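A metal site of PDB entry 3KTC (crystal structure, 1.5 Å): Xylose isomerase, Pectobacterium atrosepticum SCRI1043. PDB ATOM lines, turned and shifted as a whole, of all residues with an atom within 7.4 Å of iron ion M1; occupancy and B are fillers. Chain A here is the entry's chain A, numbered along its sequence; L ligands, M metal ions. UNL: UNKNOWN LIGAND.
Within 4 Å of iron ion M1: Glu 167, Asp 202, Asp 230 and Asp 271.
The side-chain amino group of Lys 125 lies within salt-bridge range of the side-chain carboxylate of Glu 167 (3.5 Å).
OD1 of Asp 202 sits at hydrogen-bond distance from N of His 205 (3.1 Å).
The side-chain carboxylate (OD1) of Asp 202 lies within hydrogen-bond range of the backbone NH (N) of Gly 204.
The backbone NH (N) of Asp 230 sits at hydrogen-bond distance from the backbone carbonyl oxygen (O) of Leu 201 (3.0 Å).
N of Phe 203 is in hydrogen-bond range of O of Asp 230 (2.9 Å).
The backbone carbonyl oxygen of Asp 271 sits at hydrogen-bond distance from the side-chain amide nitrogen of Asn 232, at 3.0 Å.
The backbone carbonyl oxygen (O) of Val 231 sits at hydrogen-bond distance from the backbone NH (N) of Asp 271.
OD1 of Asp 202 is in hydrogen-bond range of ND2 of Asn 232.
Iron ion M1 is bound by OD2 of Asp 271 (1.9 Å), OE2 of Glu 167 (2.0 Å), OD2 of Asp 230 (2.1 Å) and OD2 of Asp 202 (2.2 Å).
Slightly farther from iron ion M1 lies O3 of the ligand (2.6 Å).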
ATOM      1  N   TRP A  15     -23.122   1.300 -34.007  1.00  0.00           N
ATOM      2  CA  TRP A  15     -22.601   2.648 -34.153  1.00  0.00           C
ATOM      3  C   TRP A  15     -21.501   2.779 -35.206  1.00  0.00           C
ATOM      4  O   TRP A  15     -21.189   3.882 -35.607  1.00  0.00           O
ATOM      5  CB  TRP A  15     -22.098   3.179 -32.812  1.00  0.00           C
ATOM      6  CG  TRP A  15     -21.000   2.327 -32.236  1.00  0.00           C
ATOM      7  CD1 TRP A  15     -19.669   2.448 -32.476  1.00  0.00           C
ATOM      8  CD2 TRP A  15     -21.156   1.199 -31.358  1.00  0.00           C
ATOM      9  NE1 TRP A  15     -18.987   1.481 -31.806  1.00  0.00           N
ATOM     10  CE2 TRP A  15     -19.864   0.692 -31.110  1.00  0.00           C
ATOM     11  CE3 TRP A  15     -22.260   0.565 -30.772  1.00  0.00           C
ATOM     12  CZ2 TRP A  15     -19.640  -0.410 -30.291  1.00  0.00           C
ATOM     13  CZ3 TRP A  15     -22.042  -0.528 -29.975  1.00  0.00           C
ATOM     14  CH2 TRP A  15     -20.740  -1.006 -29.731  1.00  0.00           C
ATOM     15  N   LYS A 125     -23.332  -5.195 -22.665  1.00  0.00           N
ATOM     16  CA  LYS A 125     -21.998  -4.607 -22.826  1.00  0.00           C
ATOM     17  C   LYS A 125     -21.986  -3.309 -22.001  1.00  0.00           C
ATOM     18  O   LYS A 125     -22.664  -2.337 -22.336  1.00  0.00           O
ATOM     19  CB  LYS A 125     -21.767  -4.335 -24.298  1.00  0.00           C
ATOM     20  CG  LYS A 125     -20.327  -4.297 -24.714  1.00  0.00           C
ATOM     21  CD  LYS A 125     -19.564  -3.103 -24.280  1.00  0.00           C
ATOM     22  CE  LYS A 125     -20.079  -1.777 -24.877  1.00  0.00           C
ATOM     23  NZ  LYS A 125     -20.225  -1.787 -26.358  1.00  0.00           N
ATOM     24  N   TRP A 127     -20.192  -0.170 -20.631  1.00  0.00           N
ATOM     25  CA  TRP A 127     -19.095   0.788 -20.835  1.00  0.00           C
ATOM     26  C   TRP A 127     -19.461   2.083 -20.154  1.00  0.00           C
ATOM     27  O   TRP A 127     -20.162   2.893 -20.703  1.00  0.00           O
ATOM     28  CB  TRP A 127     -18.820   1.055 -22.309  1.00  0.00           C
ATOM     29  CG  TRP A 127     -17.732   2.047 -22.453  1.00  0.00           C
ATOM     30  CD1 TRP A 127     -16.412   1.881 -22.135  1.00  0.00           C
ATOM     31  CD2 TRP A 127     -17.862   3.394 -22.909  1.00  0.00           C
ATOM     32  NE1 TRP A 127     -15.724   3.045 -22.363  1.00  0.00           N
ATOM     33  CE2 TRP A 127     -16.597   4.000 -22.818  1.00  0.00           C
ATOM     34  CE3 TRP A 127     -18.945   4.167 -23.340  1.00  0.00           C
ATOM     35  CZ2 TRP A 127     -16.373   5.329 -23.183  1.00  0.00           C
ATOM     36  CZ3 TRP A 127     -18.725   5.462 -23.722  1.00  0.00           C
ATOM     37  CH2 TRP A 127     -17.457   6.034 -23.641  1.00  0.00           C
ATOM     38  N   GLU A 167     -16.406  -3.258 -20.625  1.00  0.00           N
ATOM     39  CA  GLU A 167     -15.436  -2.786 -21.603  1.00  0.00           C
ATOM     40  C   GLU A 167     -14.518  -1.774 -20.972  1.00  0.00           C
ATOM     41  O   GLU A 167     -14.869  -0.606 -20.833  1.00  0.00           O
ATOM     42  CB  GLU A 167     -16.121  -2.200 -22.847  1.00  0.00           C
ATOM     43  CG  GLU A 167     -15.113  -1.789 -23.863  1.00  0.00           C
ATOM     44  CD  GLU A 167     -15.725  -1.404 -25.152  1.00  0.00           C
ATOM     45  OE1 GLU A 167     -16.934  -1.131 -25.212  1.00  0.00           O
ATOM     46  OE2 GLU A 167     -14.973  -1.317 -26.124  1.00  0.00           O
ATOM     47  N   TYR A 168     -13.363  -2.218 -20.536  1.00  0.00           N
ATOM     48  CA  TYR A 168     -12.438  -1.269 -19.956  1.00  0.00           C
ATOM     49  C   TYR A 168     -11.878  -0.321 -21.005  1.00  0.00           C
ATOM     50  O   TYR A 168     -11.843  -0.622 -22.178  1.00  0.00           O
ATOM     51  CB  TYR A 168     -11.310  -1.980 -19.221  1.00  0.00           C
ATOM     52  CG  TYR A 168     -10.294  -2.722 -20.039  1.00  0.00           C
ATOM     53  CD1 TYR A 168      -9.186  -2.061 -20.579  1.00  0.00           C
ATOM     54  CD2 TYR A 168     -10.389  -4.082 -20.243  1.00  0.00           C
ATOM     55  CE1 TYR A 168      -8.201  -2.727 -21.304  1.00  0.00           C
ATOM     56  CE2 TYR A 168      -9.416  -4.763 -20.958  1.00  0.00           C
ATOM     57  CZ  TYR A 168      -8.336  -4.093 -21.497  1.00  0.00           C
ATOM     58  OH  TYR A 168      -7.357  -4.831 -22.156  1.00  0.00           O
ATOM     59  N   LYS A 169     -11.449   0.849 -20.545  1.00  0.00           N
ATOM     60  CA  LYS A 169     -10.929   1.880 -21.402  1.00  0.00           C
ATOM     61  C   LYS A 169     -10.107   2.831 -20.535  1.00  0.00           C
ATOM     62  O   LYS A 169     -10.548   3.176 -19.467  1.00  0.00           O
ATOM     63  CB  LYS A 169     -12.058   2.651 -22.094  1.00  0.00           C
ATOM     64  CG  LYS A 169     -11.595   3.519 -23.248  1.00  0.00           C
ATOM     65  CD  LYS A 169     -12.713   4.391 -23.739  1.00  0.00           C
ATOM     66  CE  LYS A 169     -12.267   5.231 -24.910  1.00  0.00           C
ATOM     67  NZ  LYS A 169     -13.339   6.192 -25.329  1.00  0.00           N
ATOM     68  N   LEU A 200     -15.111  -7.225 -21.923  1.00  0.00           N
ATOM     69  CA  LEU A 200     -15.114  -6.968 -23.369  1.00  0.00           C
ATOM     70  C   LEU A 200     -13.746  -6.310 -23.627  1.00  0.00           C
ATOM     71  O   LEU A 200     -13.505  -5.182 -23.226  1.00  0.00           O
ATOM     72  CB  LEU A 200     -16.266  -6.050 -23.755  1.00  0.00           C
ATOM     73  CG  LEU A 200     -16.649  -5.918 -25.237  1.00  0.00           C
ATOM     74  CD1 LEU A 200     -15.462  -5.501 -26.102  1.00  0.00           C
ATOM     75  CD2 LEU A 200     -17.310  -7.200 -25.753  1.00  0.00           C
ATOM     76  N   LEU A 201     -12.847  -7.041 -24.273  1.00  0.00           N
ATOM     77  CA  LEU A 201     -11.464  -6.565 -24.510  1.00  0.00           C
ATOM     78  C   LEU A 201     -11.420  -5.885 -25.861  1.00  0.00           C
ATOM     79  O   LEU A 201     -11.583  -6.544 -26.883  1.00  0.00           O
ATOM     80  CB  LEU A 201     -10.488  -7.754 -24.477  1.00  0.00           C
ATOM     81  CG  LEU A 201      -8.998  -7.459 -24.335  1.00  0.00           C
ATOM     82  CD1 LEU A 201      -8.237  -8.783 -24.470  1.00  0.00           C
ATOM     83  CD2 LEU A 201      -8.431  -6.414 -25.283  1.00  0.00           C
ATOM     84  N   ASP A 202     -11.258  -4.576 -25.855  1.00  0.00           N
ATOM     85  CA  ASP A 202     -11.139  -3.773 -27.070  1.00  0.00           C
ATOM     86  C   ASP A 202      -9.656  -3.662 -27.326  1.00  0.00           C
ATOM     87  O   ASP A 202      -8.902  -3.091 -26.522  1.00  0.00           O
ATOM     88  CB  ASP A 202     -11.840  -2.429 -26.877  1.00  0.00           C
ATOM     89  CG  ASP A 202     -11.800  -1.549 -28.110  1.00  0.00           C
ATOM     90  OD1 ASP A 202     -10.705  -1.345 -28.671  1.00  0.00           O
ATOM     91  OD2 ASP A 202     -12.868  -1.006 -28.471  1.00  0.00           O
ATOM     92  N   PHE A 203      -9.221  -4.245 -28.436  1.00  0.00           N
ATOM     93  CA  PHE A 203      -7.801  -4.226 -28.805  1.00  0.00           C
ATOM     94  C   PHE A 203      -7.224  -2.815 -28.763  1.00  0.00           C
ATOM     95  O   PHE A 203      -6.107  -2.601 -28.270  1.00  0.00           O
ATOM     96  CB  PHE A 203      -7.631  -4.815 -30.195  1.00  0.00           C
ATOM     97  CG  PHE A 203      -6.256  -4.621 -30.775  1.00  0.00           C
ATOM     98  CD1 PHE A 203      -5.267  -5.564 -30.559  1.00  0.00           C
ATOM     99  CD2 PHE A 203      -5.939  -3.488 -31.544  1.00  0.00           C
ATOM    100  CE1 PHE A 203      -4.006  -5.400 -31.099  1.00  0.00           C
ATOM    101  CE2 PHE A 203      -4.670  -3.348 -32.082  1.00  0.00           C
ATOM    102  CZ  PHE A 203      -3.704  -4.297 -31.813  1.00  0.00           C
ATOM    103  N   GLY A 204      -7.948  -1.851 -29.329  1.00  0.00           N
ATOM    104  CA  GLY A 204      -7.490  -0.478 -29.374  1.00  0.00           C
ATOM    105  C   GLY A 204      -7.330   0.140 -27.990  1.00  0.00           C
ATOM    106  O   GLY A 204      -6.386   0.887 -27.736  1.00  0.00           O
ATOM    107  N   HIS A 205      -8.252  -0.179 -27.092  1.00  0.00           N
ATOM    108  CA  HIS A 205      -8.174   0.327 -25.717  1.00  0.00           C
ATOM    109  C   HIS A 205      -6.955  -0.219 -25.030  1.00  0.00           C
ATOM    110  O   HIS A 205      -6.214   0.529 -24.354  1.00  0.00           O
ATOM    111  CB  HIS A 205      -9.431  -0.024 -24.926  1.00  0.00           C
ATOM    112  CG  HIS A 205     -10.679   0.618 -25.457  1.00  0.00           C
ATOM    113  ND1 HIS A 205     -11.890   0.484 -24.818  1.00  0.00           N
ATOM    114  CD2 HIS A 205     -10.895   1.413 -26.539  1.00  0.00           C
ATOM    115  CE1 HIS A 205     -12.810   1.144 -25.504  1.00  0.00           C
ATOM    116  NE2 HIS A 205     -12.242   1.693 -26.570  1.00  0.00           N
ATOM    117  N   MET A 229     -14.681  -9.510 -27.687  1.00  0.00           N
ATOM    118  CA  MET A 229     -13.604  -8.656 -28.141  1.00  0.00           C
ATOM    119  C   MET A 229     -14.177  -7.565 -29.020  1.00  0.00           C
ATOM    120  O   MET A 229     -15.273  -7.695 -29.546  1.00  0.00           O
ATOM    121  CB  MET A 229     -12.631  -9.430 -29.052  1.00  0.00           C
ATOM    122  CG  MET A 229     -13.017  -9.257 -30.624  1.00  0.00           C
ATOM    123  SD  MET A 229     -12.101  -9.963 -31.710  1.00  0.00           S
ATOM    124  CE  MET A 229     -12.491 -11.894 -31.395  1.00  0.00           C
ATOM    125  N   ASP A 230     -13.386  -6.520 -29.248  1.00  0.00           N
ATOM    126  CA  ASP A 230     -13.635  -5.432 -30.221  1.00  0.00           C
ATOM    127  C   ASP A 230     -12.261  -5.231 -30.902  1.00  0.00           C
ATOM    128  O   ASP A 230     -11.237  -5.266 -30.215  1.00  0.00           O
ATOM    129  CB  ASP A 230     -13.976  -4.067 -29.507  1.00  0.00           C
ATOM    130  CG  ASP A 230     -15.470  -3.822 -29.315  1.00  0.00           C
ATOM    131  OD1 ASP A 230     -16.297  -4.448 -30.007  1.00  0.00           O
ATOM    132  OD2 ASP A 230     -15.820  -2.938 -28.499  1.00  0.00           O
ATOM    133  N   VAL A 231     -12.215  -4.972 -32.223  1.00  0.00           N
ATOM    134  CA  VAL A 231     -10.958  -4.589 -32.875  1.00  0.00           C
ATOM    135  C   VAL A 231     -11.132  -3.296 -33.650  1.00  0.00           C
ATOM    136  O   VAL A 231     -12.230  -2.912 -34.011  1.00  0.00           O
ATOM    137  CB  VAL A 231     -10.362  -5.690 -33.747  1.00  0.00           C
ATOM    138  CG1 VAL A 231     -10.090  -6.923 -32.844  1.00  0.00           C
ATOM    139  CG2 VAL A 231     -11.282  -6.037 -34.916  1.00  0.00           C
ATOM    140  N   ASN A 232      -9.976  -2.671 -33.896  1.00  0.00           N
ATOM    141  CA  ASN A 232      -9.819  -1.344 -34.499  1.00  0.00           C
ATOM    142  C   ASN A 232      -8.317  -1.075 -34.434  1.00  0.00           C
ATOM    143  O   ASN A 232      -7.544  -1.944 -34.047  1.00  0.00           O
ATOM    144  CB  ASN A 232     -10.611  -0.260 -33.747  1.00  0.00           C
ATOM    145  CG  ASN A 232     -10.339  -0.252 -32.282  1.00  0.00           C
ATOM    146  OD1 ASN A 232      -9.260   0.147 -31.845  1.00  0.00           O
ATOM    147  ND2 ASN A 232     -11.307  -0.721 -31.497  1.00  0.00           N
ATOM    148  N   ASP A 239      -7.968   6.670 -28.326  1.00  0.00           N
ATOM    149  CA  ASP A 239      -8.914   5.705 -28.917  1.00  0.00           C
ATOM    150  C   ASP A 239      -9.334   6.182 -30.303  1.00  0.00           C
ATOM    151  O   ASP A 239     -10.480   6.612 -30.530  1.00  0.00           O
ATOM    152  CB  ASP A 239     -10.131   5.570 -28.006  1.00  0.00           C
ATOM    153  CG  ASP A 239     -11.021   4.417 -28.371  1.00  0.00           C
ATOM    154  OD1 ASP A 239     -10.496   3.428 -28.937  1.00  0.00           O
ATOM    155  OD2 ASP A 239     -12.251   4.481 -28.097  1.00  0.00           O
ATOM    156  N   ASP A 241      -9.940   4.670 -33.059  1.00  0.00           N
ATOM    157  CA  ASP A 241     -11.023   3.875 -33.661  1.00  0.00           C
ATOM    158  C   ASP A 241     -10.947   3.841 -35.177  1.00  0.00           C
ATOM    159  O   ASP A 241     -11.952   3.912 -35.863  1.00  0.00           O
ATOM    160  CB  ASP A 241     -12.389   4.386 -33.183  1.00  0.00           C
ATOM    161  CG  ASP A 241     -12.693   3.993 -31.763  1.00  0.00           C
ATOM    162  OD1 ASP A 241     -12.301   2.894 -31.341  1.00  0.00           O
ATOM    163  OD2 ASP A 241     -13.397   4.770 -31.093  1.00  0.00           O
ATOM    164  N   GLN A 269     -15.289  -8.949 -33.848  1.00  0.00           N
ATOM    165  CA  GLN A 269     -16.155  -7.799 -33.755  1.00  0.00           C
ATOM    166  C   GLN A 269     -15.440  -6.469 -33.949  1.00  0.00           C
ATOM    167  O   GLN A 269     -14.455  -6.173 -33.271  1.00  0.00           O
ATOM    168  CB  GLN A 269     -16.802  -7.831 -32.383  1.00  0.00           C
ATOM    169  CG  GLN A 269     -17.784  -6.699 -32.023  1.00  0.00           C
ATOM    170  CD  GLN A 269     -19.203  -6.927 -32.492  1.00  0.00           C
ATOM    171  OE1 GLN A 269     -19.524  -7.967 -33.056  1.00  0.00           O
ATOM    172  NE2 GLN A 269     -20.060  -5.941 -32.266  1.00  0.00           N
ATOM    173  N   LEU A 270     -15.982  -5.644 -34.840  1.00  0.00           N
ATOM    174  CA  LEU A 270     -15.391  -4.340 -35.129  1.00  0.00           C
ATOM    175  C   LEU A 270     -15.996  -3.265 -34.238  1.00  0.00           C
ATOM    176  O   LEU A 270     -17.216  -3.203 -34.094  1.00  0.00           O
ATOM    177  CB  LEU A 270     -15.707  -3.947 -36.568  1.00  0.00           C
ATOM    178  CG  LEU A 270     -15.306  -4.895 -37.702  1.00  0.00           C
ATOM    179  CD1 LEU A 270     -15.797  -4.344 -39.041  1.00  0.00           C
ATOM    180  CD2 LEU A 270     -13.803  -5.045 -37.664  1.00  0.00           C
ATOM    181  N   ASP A 271     -15.161  -2.431 -33.630  1.00  0.00           N
ATOM    182  CA  ASP A 271     -15.639  -1.227 -32.951  1.00  0.00           C
ATOM    183  C   ASP A 271     -14.805  -0.086 -33.515  1.00  0.00           C
ATOM    184  O   ASP A 271     -13.694   0.203 -33.031  1.00  0.00           O
ATOM    185  CB  ASP A 271     -15.462  -1.351 -31.441  1.00  0.00           C
ATOM    186  CG  ASP A 271     -15.847  -0.095 -30.704  1.00  0.00           C
ATOM    187  OD1 ASP A 271     -16.349   0.850 -31.334  1.00  0.00           O
ATOM    188  OD2 ASP A 271     -15.648  -0.036 -29.490  1.00  0.00           O
ATOM    189  N   GLN A 272     -15.365   0.565 -34.541  1.00  0.00           N
ATOM    190  CA  GLN A 272     -14.642   1.572 -35.324  1.00  0.00           C
ATOM    191  C   GLN A 272     -15.571   2.722 -35.591  1.00  0.00           C
ATOM    192  O   GLN A 272     -16.781   2.525 -35.672  1.00  0.00           O
ATOM    193  CB  GLN A 272     -14.162   0.944 -36.638  1.00  0.00           C
ATOM    194  CG  GLN A 272     -13.147  -0.171 -36.382  1.00  0.00           C
ATOM    195  CD  GLN A 272     -12.779  -1.059 -37.542  1.00  0.00           C
ATOM    196  OE1 GLN A 272     -11.740  -1.729 -37.456  1.00  0.00           O
ATOM    197  NE2 GLN A 272     -13.561  -1.088 -38.632  1.00  0.00           N
ATOM    198  N   PHE A 273     -14.995   3.902 -35.742  1.00  0.00           N
ATOM    199  CA  PHE A 273     -15.737   5.141 -35.998  1.00  0.00           C
ATOM    200  C   PHE A 273     -15.188   5.807 -37.255  1.00  0.00           C
ATOM    201  O   PHE A 273     -14.275   6.612 -37.177  1.00  0.00           O
ATOM    202  CB  PHE A 273     -15.562   6.137 -34.833  1.00  0.00           C
ATOM    203  CG  PHE A 273     -16.429   5.838 -33.605  1.00  0.00           C
ATOM    204  CD1 PHE A 273     -16.215   4.734 -32.821  1.00  0.00           C
ATOM    205  CD2 PHE A 273     -17.433   6.726 -33.214  1.00  0.00           C
ATOM    206  CE1 PHE A 273     -17.007   4.491 -31.691  1.00  0.00           C
ATOM    207  CE2 PHE A 273     -18.209   6.487 -32.100  1.00  0.00           C
ATOM    208  CZ  PHE A 273     -18.000   5.370 -31.342  1.00  0.00           C
HETATM  209  O1  UNL L   1     -16.251   2.391 -26.266  1.00  0.00           O
HETATM  210  O2  UNL L   1     -14.837   3.788 -26.318  1.00  0.00           O
HETATM  211  O3  UNL L   1     -15.205   1.467 -27.314  1.00  0.00           O
HETATM  212  O4  UNL L   1     -17.493   0.194 -27.220  1.00  0.00           O
HETATM  213  O5  UNL L   1     -17.288   2.537 -28.830  1.00  0.00           O
HETATM  214  O6  UNL L   1     -20.048   1.174 -26.871  1.00  0.00           O
HETATM  215  O7  UNL L   1     -22.009   2.840 -27.748  1.00  0.00           O
HETATM  216  O8  UNL L   1     -21.883   3.981 -29.255  1.00  0.00           O
HETATM  217  O9  UNL L   1     -20.736   4.877 -28.391  1.00  0.00           O
HETATM  218 FE    FE M   1     -14.984  -1.035 -28.072  1.00  0.00          FE
HETATM  219 FE    FE M   2     -12.613   2.553 -29.077  1.00  0.00          FE
